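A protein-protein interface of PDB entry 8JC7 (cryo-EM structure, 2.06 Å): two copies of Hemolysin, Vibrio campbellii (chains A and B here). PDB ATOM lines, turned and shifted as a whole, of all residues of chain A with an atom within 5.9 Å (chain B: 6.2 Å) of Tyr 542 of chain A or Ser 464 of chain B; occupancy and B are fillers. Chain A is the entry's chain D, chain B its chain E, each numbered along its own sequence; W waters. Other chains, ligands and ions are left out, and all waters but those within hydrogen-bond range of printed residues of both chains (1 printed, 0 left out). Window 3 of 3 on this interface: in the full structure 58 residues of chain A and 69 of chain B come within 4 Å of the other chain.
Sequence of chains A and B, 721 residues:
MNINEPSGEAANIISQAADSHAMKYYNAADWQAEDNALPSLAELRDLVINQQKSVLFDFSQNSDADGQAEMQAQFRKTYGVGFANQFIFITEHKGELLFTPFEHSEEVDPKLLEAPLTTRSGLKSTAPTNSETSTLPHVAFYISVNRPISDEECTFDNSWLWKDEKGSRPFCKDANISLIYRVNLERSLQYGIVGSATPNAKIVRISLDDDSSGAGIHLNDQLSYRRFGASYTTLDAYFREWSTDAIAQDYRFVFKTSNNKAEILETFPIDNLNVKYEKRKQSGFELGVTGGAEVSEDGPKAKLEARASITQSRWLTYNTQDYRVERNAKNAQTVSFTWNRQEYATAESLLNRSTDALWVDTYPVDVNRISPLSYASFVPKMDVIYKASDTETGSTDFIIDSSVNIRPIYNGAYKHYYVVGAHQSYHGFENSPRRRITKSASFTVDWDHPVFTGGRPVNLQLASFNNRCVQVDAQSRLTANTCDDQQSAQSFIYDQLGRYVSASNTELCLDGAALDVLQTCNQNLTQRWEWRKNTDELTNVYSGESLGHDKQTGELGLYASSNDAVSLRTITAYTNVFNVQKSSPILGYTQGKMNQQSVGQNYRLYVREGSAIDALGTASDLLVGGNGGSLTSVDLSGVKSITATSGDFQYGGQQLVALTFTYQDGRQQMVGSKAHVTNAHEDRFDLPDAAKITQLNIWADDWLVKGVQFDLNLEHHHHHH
The backbone NH of Leu 525 of chain A is in hydrogen-bond range of the backbone carbonyl oxygen of Asn 466 of chain B (3.0 Å).
NH2 of Arg 569 of chain B sits at hydrogen-bond distance from O of Val 541 of chain A (2.7 Å).
The side-chain hydroxyl (OH) of Tyr 542 of chain A sits at hydrogen-bond distance from the backbone carbonyl oxygen (O) of Ser 464 of chain B (3.2 Å).
The side-chain amide oxygen of Asn 466 of chain B lies within hydrogen-bond range of the backbone NH of Thr 526 of chain A (3.1 Å).
NH2 of Arg 528 of chain A lies within hydrogen-bond range of OE1 of Gln 461 of chain B, at 2.9 Å.
The backbone carbonyl oxygen (O) of Tyr 542 of chain A sits at hydrogen-bond distance from the guanidinium group (NH1) of Arg 569 of chain B, 3.1 Å away.
The backbone carbonyl oxygen (O) of Thr 526 of chain A lies within hydrogen-bond range of the side-chain amide nitrogen (ND2) of Asn 540 of chain A (2.8 Å).
OG of Ser 464 of chain B lies close to NE2 of His 549 of chain B, 3.4 Å away.
The backbone carbonyl oxygen (O) of Arg 528 of chain A is in hydrogen-bond range of the backbone NH (N) of Val 541 of chain A, 2.9 Å away.
The backbone NH of Ala 463 of chain B lies within hydrogen-bond range of the backbone carbonyl oxygen of Arg 569 of chain B (3.0 Å).
OG of Ser 567 of chain B is in hydrogen-bond range of N of Arg 569 of chain B.
The backbone carbonyl oxygen of Arg 528 of chain A lies within hydrogen-bond range of the side-chain amide nitrogen of Asn 540 of chain A, at 3.2 Å.
CG of Leu 525 of chain A touches NE2 of Gln 461 of chain B (3.8 Å).
Leu 525 of chain A touches Ala 463 of chain B.
Phe 465 of chain B touches Leu 525 of chain A (O to CD1, 3.6 Å).
Tyr 542 of chain A touches Ala 463 of chain B.
Tyr 542 of chain A touches Phe 465 of chain B.
Tyr 542 of chain A touches Asn 466 of chain B.
Printed residues of chain B within 4 Å of Leu 525 of chain A: Gln 461 (3.8 Å), Ala 463 (3.7 Å), Phe 465 (3.6 Å) and Asn 466 (3.0 Å).
Of the printed residues of chain B, Arg 528 of chain A touches Gln 461.
Of chain B, only Ala 463, Ser 464, Phe 465, Asn 466 and Arg 569 come within 4 Å of Tyr 542 of chain A.
Leu 462 of chain B touches none of the printed residues of chain A.
Printed residues of chain A within 4 Å of Ala 463 of chain B: Leu 525 (3.7 Å) and Tyr 542 (3.8 Å).
Ser 464 of chain B touches just one residue of chain A: Tyr 542.
Of the printed residues of chain A, Phe 465 of chain B touches Leu 525 and Tyr 542.
Of the printed residues of chain A, Asn 466 of chain B touches Leu 525 (3.0 Å), Thr 526 (3.1 Å) and Tyr 542 (3.9 Å).
Ser 567 of chain B touches none of the printed residues of chain A.
The nearest printed residue of chain B that does not touch Tyr 542 of chain A is Leu 462 of chain B (6.5 Å).
Printed residues of chain A that touch a printed residue of chain B: Leu 525, Thr 526, Arg 528, Val 541 and Tyr 542.
Hydrophobic or aromatic side chains of chain A that line the printed part of chain B: Leu 525, Val 541 and Tyr 542.
Of the 12 printed residues of chain B, 6 touch a printed residue of chain A.
Hydrophobic or aromatic side chains of chain B that line the printed part of chain A: Ala 463.
Among the printed residues, no Asp or Glu carboxylate lies within 4 Å of a Lys or Arg side-chain nitrogen of the other chain.
No position is printed for both chains.
Of the 12 pairs that touch across the chains among the printed residues, none has its exchanged pair printed and touching as well.
Water W1 bridges the side-chain amide oxygen (OE1) of Gln 461 of chain B (2.7 Å) and the guanidinium group (NH1) of Arg 528 of chain A (3.3 Å).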
ATOM      1  N   LEU A 525      22.306 -19.671  -1.819  1.00  0.00           N
ATOM      2  CA  LEU A 525      21.156 -18.814  -2.032  1.00  0.00           C
ATOM      3  C   LEU A 525      21.116 -17.667  -1.040  1.00  0.00           C
ATOM      4  O   LEU A 525      20.492 -16.646  -1.321  1.00  0.00           O
ATOM      5  CB  LEU A 525      19.874 -19.628  -1.950  1.00  0.00           C
ATOM      6  CG  LEU A 525      19.653 -20.595  -3.101  1.00  0.00           C
ATOM      7  CD1 LEU A 525      18.334 -21.272  -2.933  1.00  0.00           C
ATOM      8  CD2 LEU A 525      19.703 -19.865  -4.411  1.00  0.00           C
ATOM      9  N   THR A 526      21.772 -17.808   0.107  1.00  0.00           N
ATOM     10  CA  THR A 526      21.855 -16.711   1.053  1.00  0.00           C
ATOM     11  C   THR A 526      22.741 -15.582   0.562  1.00  0.00           C
ATOM     12  O   THR A 526      22.732 -14.508   1.165  1.00  0.00           O
ATOM     13  CB  THR A 526      22.376 -17.198   2.394  1.00  0.00           C
ATOM     14  OG1 THR A 526      23.557 -17.973   2.190  1.00  0.00           O
ATOM     15  CG2 THR A 526      21.346 -18.043   3.076  1.00  0.00           C
ATOM     16  N   ARG A 528      22.380 -14.278  -2.456  1.00  0.00           N
ATOM     17  CA  ARG A 528      21.653 -13.627  -3.529  1.00  0.00           C
ATOM     18  C   ARG A 528      20.619 -12.686  -2.942  1.00  0.00           C
ATOM     19  O   ARG A 528      19.927 -13.037  -1.984  1.00  0.00           O
ATOM     20  CB  ARG A 528      20.995 -14.654  -4.437  1.00  0.00           C
ATOM     21  CG  ARG A 528      21.994 -15.490  -5.163  1.00  0.00           C
ATOM     22  CD  ARG A 528      21.335 -16.468  -6.065  1.00  0.00           C
ATOM     23  NE  ARG A 528      22.157 -17.653  -6.213  1.00  0.00           N
ATOM     24  CZ  ARG A 528      21.928 -18.606  -7.098  1.00  0.00           C
ATOM     25  NH1 ARG A 528      20.898 -18.512  -7.915  1.00  0.00           N
ATOM     26  NH2 ARG A 528      22.729 -19.650  -7.160  1.00  0.00           N
ATOM     27  N   ASN A 540      16.683 -11.155   0.978  1.00  0.00           N
ATOM     28  CA  ASN A 540      17.493 -12.324   0.692  1.00  0.00           C
ATOM     29  C   ASN A 540      16.690 -13.335  -0.109  1.00  0.00           C
ATOM     30  O   ASN A 540      15.511 -13.562   0.161  1.00  0.00           O
ATOM     31  CB  ASN A 540      17.975 -12.952   1.990  1.00  0.00           C
ATOM     32  CG  ASN A 540      19.191 -13.797   1.802  1.00  0.00           C
ATOM     33  OD1 ASN A 540      19.230 -14.940   2.231  1.00  0.00           O
ATOM     34  ND2 ASN A 540      20.201 -13.244   1.163  1.00  0.00           N
ATOM     35  N   VAL A 541      17.333 -13.944  -1.099  1.00  0.00           N
ATOM     36  CA  VAL A 541      16.626 -14.867  -1.977  1.00  0.00           C
ATOM     37  C   VAL A 541      16.264 -16.146  -1.238  1.00  0.00           C
ATOM     38  O   VAL A 541      15.180 -16.702  -1.432  1.00  0.00           O
ATOM     39  CB  VAL A 541      17.466 -15.149  -3.233  1.00  0.00           C
ATOM     40  CG1 VAL A 541      17.066 -16.458  -3.858  1.00  0.00           C
ATOM     41  CG2 VAL A 541      17.300 -14.028  -4.219  1.00  0.00           C
ATOM     42  N   TYR A 542      17.154 -16.631  -0.378  1.00  0.00           N
ATOM     43  CA  TYR A 542      16.937 -17.926   0.253  1.00  0.00           C
ATOM     44  C   TYR A 542      15.713 -17.917   1.153  1.00  0.00           C
ATOM     45  O   TYR A 542      14.828 -18.766   1.024  1.00  0.00           O
ATOM     46  CB  TYR A 542      18.169 -18.326   1.052  1.00  0.00           C
ATOM     47  CG  TYR A 542      18.032 -19.652   1.734  1.00  0.00           C
ATOM     48  CD1 TYR A 542      17.619 -20.768   1.036  1.00  0.00           C
ATOM     49  CD2 TYR A 542      18.321 -19.793   3.074  1.00  0.00           C
ATOM     50  CE1 TYR A 542      17.498 -21.981   1.651  1.00  0.00           C
ATOM     51  CE2 TYR A 542      18.203 -21.002   3.696  1.00  0.00           C
ATOM     52  CZ  TYR A 542      17.792 -22.093   2.981  1.00  0.00           C
ATOM     53  OH  TYR A 542      17.670 -23.306   3.603  1.00  0.00           O
ATOM     54  N   SER A 543      15.641 -16.961   2.075  1.00  0.00           N
ATOM     55  CA  SER A 543      14.590 -16.954   3.077  1.00  0.00           C
ATOM     56  C   SER A 543      13.509 -15.923   2.830  1.00  0.00           C
ATOM     57  O   SER A 543      12.449 -16.009   3.453  1.00  0.00           O
ATOM     58  CB  SER A 543      15.185 -16.709   4.468  1.00  0.00           C
ATOM     59  OG  SER A 543      16.079 -15.614   4.442  1.00  0.00           O
ATOM     60  N   GLY A 544      13.743 -14.955   1.957  1.00  0.00           N
ATOM     61  CA  GLY A 544      12.793 -13.890   1.752  1.00  0.00           C
ATOM     62  C   GLY A 544      12.853 -12.793   2.784  1.00  0.00           C
ATOM     63  O   GLY A 544      12.115 -11.812   2.661  1.00  0.00           O
ATOM     64  N   GLN B 461      18.956 -25.541  -9.417  1.00  0.00           N
ATOM     65  CA  GLN B 461      19.280 -25.479  -8.006  1.00  0.00           C
ATOM     66  C   GLN B 461      18.045 -25.799  -7.181  1.00  0.00           C
ATOM     67  O   GLN B 461      16.992 -25.195  -7.374  1.00  0.00           O
ATOM     68  CB  GLN B 461      19.819 -24.100  -7.651  1.00  0.00           C
ATOM     69  CG  GLN B 461      20.383 -24.004  -6.272  1.00  0.00           C
ATOM     70  CD  GLN B 461      21.490 -23.001  -6.185  1.00  0.00           C
ATOM     71  OE1 GLN B 461      21.860 -22.387  -7.175  1.00  0.00           O
ATOM     72  NE2 GLN B 461      22.030 -22.824  -4.995  1.00  0.00           N
ATOM     73  N   LEU B 462      18.176 -26.756  -6.274  1.00  0.00           N
ATOM     74  CA  LEU B 462      17.077 -27.125  -5.394  1.00  0.00           C
ATOM     75  C   LEU B 462      17.011 -26.105  -4.271  1.00  0.00           C
ATOM     76  O   LEU B 462      17.860 -26.100  -3.379  1.00  0.00           O
ATOM     77  CB  LEU B 462      17.276 -28.536  -4.862  1.00  0.00           C
ATOM     78  CG  LEU B 462      17.639 -29.524  -5.963  1.00  0.00           C
ATOM     79  CD1 LEU B 462      17.836 -30.895  -5.394  1.00  0.00           C
ATOM     80  CD2 LEU B 462      16.560 -29.541  -7.011  1.00  0.00           C
ATOM     81  N   ALA B 463      16.003 -25.248  -4.308  1.00  0.00           N
ATOM     82  CA  ALA B 463      16.014 -24.033  -3.515  1.00  0.00           C
ATOM     83  C   ALA B 463      15.565 -24.233  -2.080  1.00  0.00           C
ATOM     84  O   ALA B 463      15.552 -23.264  -1.322  1.00  0.00           O
ATOM     85  CB  ALA B 463      15.148 -22.969  -4.177  1.00  0.00           C
ATOM     86  N   SER B 464      15.182 -25.440  -1.681  1.00  0.00           N
ATOM     87  CA  SER B 464      14.964 -25.670  -0.260  1.00  0.00           C
ATOM     88  C   SER B 464      16.283 -25.745   0.490  1.00  0.00           C
ATOM     89  O   SER B 464      16.329 -25.465   1.689  1.00  0.00           O
ATOM     90  CB  SER B 464      14.163 -26.946  -0.042  1.00  0.00           C
ATOM     91  OG  SER B 464      15.007 -28.001   0.369  1.00  0.00           O
ATOM     92  N   PHE B 465      17.351 -26.130  -0.190  1.00  0.00           N
ATOM     93  CA  PHE B 465      18.686 -26.127   0.377  1.00  0.00           C
ATOM     94  C   PHE B 465      19.371 -24.804   0.097  1.00  0.00           C
ATOM     95  O   PHE B 465      19.012 -24.074  -0.824  1.00  0.00           O
ATOM     96  CB  PHE B 465      19.532 -27.249  -0.204  1.00  0.00           C
ATOM     97  CG  PHE B 465      18.967 -28.603   0.006  1.00  0.00           C
ATOM     98  CD1 PHE B 465      19.258 -29.312   1.145  1.00  0.00           C
ATOM     99  CD2 PHE B 465      18.155 -29.178  -0.943  1.00  0.00           C
ATOM    100  CE1 PHE B 465      18.744 -30.557   1.334  1.00  0.00           C
ATOM    101  CE2 PHE B 465      17.642 -30.422  -0.755  1.00  0.00           C
ATOM    102  CZ  PHE B 465      17.936 -31.113   0.384  1.00  0.00           C
ATOM    103  N   ASN B 466      20.382 -24.505   0.902  1.00  0.00           N
ATOM    104  CA  ASN B 466      21.181 -23.323   0.629  1.00  0.00           C
ATOM    105  C   ASN B 466      22.055 -23.525  -0.597  1.00  0.00           C
ATOM    106  O   ASN B 466      22.206 -22.611  -1.411  1.00  0.00           O
ATOM    107  CB  ASN B 466      22.031 -22.972   1.842  1.00  0.00           C
ATOM    108  CG  ASN B 466      22.556 -21.567   1.781  1.00  0.00           C
ATOM    109  OD1 ASN B 466      22.001 -20.720   1.096  1.00  0.00           O
ATOM    110  ND2 ASN B 466      23.634 -21.311   2.494  1.00  0.00           N
ATOM    111  N   HIS B 549      11.562 -31.788  -4.949  1.00  0.00           N
ATOM    112  CA  HIS B 549      12.674 -32.534  -4.401  1.00  0.00           C
ATOM    113  C   HIS B 549      12.433 -32.785  -2.927  1.00  0.00           C
ATOM    114  O   HIS B 549      11.825 -31.970  -2.234  1.00  0.00           O
ATOM    115  CB  HIS B 549      13.991 -31.802  -4.594  1.00  0.00           C
ATOM    116  CG  HIS B 549      13.990 -30.414  -4.046  1.00  0.00           C
ATOM    117  ND1 HIS B 549      13.522 -29.336  -4.758  1.00  0.00           N
ATOM    118  CD2 HIS B 549      14.398 -29.930  -2.853  1.00  0.00           C
ATOM    119  CE1 HIS B 549      13.641 -28.246  -4.028  1.00  0.00           C
ATOM    120  NE2 HIS B 549      14.170 -28.578  -2.867  1.00  0.00           N
ATOM    121  N   ASP B 550      12.901 -33.933  -2.462  1.00  0.00           N
ATOM    122  CA  ASP B 550      12.819 -34.250  -1.049  1.00  0.00           C
ATOM    123  C   ASP B 550      13.646 -33.259  -0.250  1.00  0.00           C
ATOM    124  O   ASP B 550      14.781 -32.946  -0.610  1.00  0.00           O
ATOM    125  CB  ASP B 550      13.311 -35.672  -0.810  1.00  0.00           C
ATOM    126  CG  ASP B 550      13.418 -36.007   0.653  1.00  0.00           C
ATOM    127  OD1 ASP B 550      14.351 -36.746   1.020  1.00  0.00           O
ATOM    128  OD2 ASP B 550      12.573 -35.538   1.439  1.00  0.00           O
ATOM    129  N   LYS B 551      13.073 -32.762   0.843  1.00  0.00           N
ATOM    130  CA  LYS B 551      13.731 -31.720   1.612  1.00  0.00           C
ATOM    131  C   LYS B 551      14.942 -32.217   2.381  1.00  0.00           C
ATOM    132  O   LYS B 551      15.692 -31.393   2.908  1.00  0.00           O
ATOM    133  CB  LYS B 551      12.741 -31.085   2.578  1.00  0.00           C
ATOM    134  CG  LYS B 551      11.845 -30.069   1.934  1.00  0.00           C
ATOM    135  CD  LYS B 551      11.068 -29.321   2.977  1.00  0.00           C
ATOM    136  CE  LYS B 551      10.173 -28.287   2.346  1.00  0.00           C
ATOM    137  NZ  LYS B 551       8.768 -28.452   2.783  1.00  0.00           N
ATOM    138  N   GLN B 552      15.157 -33.525   2.459  1.00  0.00           N
ATOM    139  CA  GLN B 552      16.293 -34.078   3.180  1.00  0.00           C
ATOM    140  C   GLN B 552      17.400 -34.568   2.264  1.00  0.00           C
ATOM    141  O   GLN B 552      18.576 -34.328   2.542  1.00  0.00           O
ATOM    142  CB  GLN B 552      15.838 -35.231   4.073  1.00  0.00           C
ATOM    143  CG  GLN B 552      15.657 -34.849   5.518  1.00  0.00           C
ATOM    144  CD  GLN B 552      14.502 -33.896   5.721  1.00  0.00           C
ATOM    145  OE1 GLN B 552      13.632 -33.763   4.862  1.00  0.00           O
ATOM    146  NE2 GLN B 552      14.487 -33.224   6.863  1.00  0.00           N
ATOM    147  N   SER B 567       9.681 -30.054  -1.428  1.00  0.00           N
ATOM    148  CA  SER B 567       9.688 -28.658  -1.825  1.00  0.00           C
ATOM    149  C   SER B 567       9.586 -28.560  -3.335  1.00  0.00           C
ATOM    150  O   SER B 567      10.186 -29.355  -4.057  1.00  0.00           O
ATOM    151  CB  SER B 567      10.955 -27.962  -1.348  1.00  0.00           C
ATOM    152  OG  SER B 567      11.136 -26.740  -2.030  1.00  0.00           O
ATOM    153  N   ARG B 569      10.396 -25.681  -4.982  1.00  0.00           N
ATOM    154  CA  ARG B 569      11.119 -24.477  -5.353  1.00  0.00           C
ATOM    155  C   ARG B 569      12.377 -24.844  -6.126  1.00  0.00           C
ATOM    156  O   ARG B 569      13.275 -25.492  -5.589  1.00  0.00           O
ATOM    157  CB  ARG B 569      11.474 -23.660  -4.120  1.00  0.00           C
ATOM    158  CG  ARG B 569      11.564 -22.193  -4.398  1.00  0.00           C
ATOM    159  CD  ARG B 569      12.032 -21.440  -3.191  1.00  0.00           C
ATOM    160  NE  ARG B 569      12.528 -20.124  -3.557  1.00  0.00           N
ATOM    161  CZ  ARG B 569      13.363 -19.415  -2.815  1.00  0.00           C
ATOM    162  NH1 ARG B 569      13.794 -19.896  -1.663  1.00  0.00           N
ATOM    163  NH2 ARG B 569      13.761 -18.226  -3.226  1.00  0.00           N
HETATM  164  O   HOH W   1      20.980 -21.407  -9.512  1.00  0.00           O
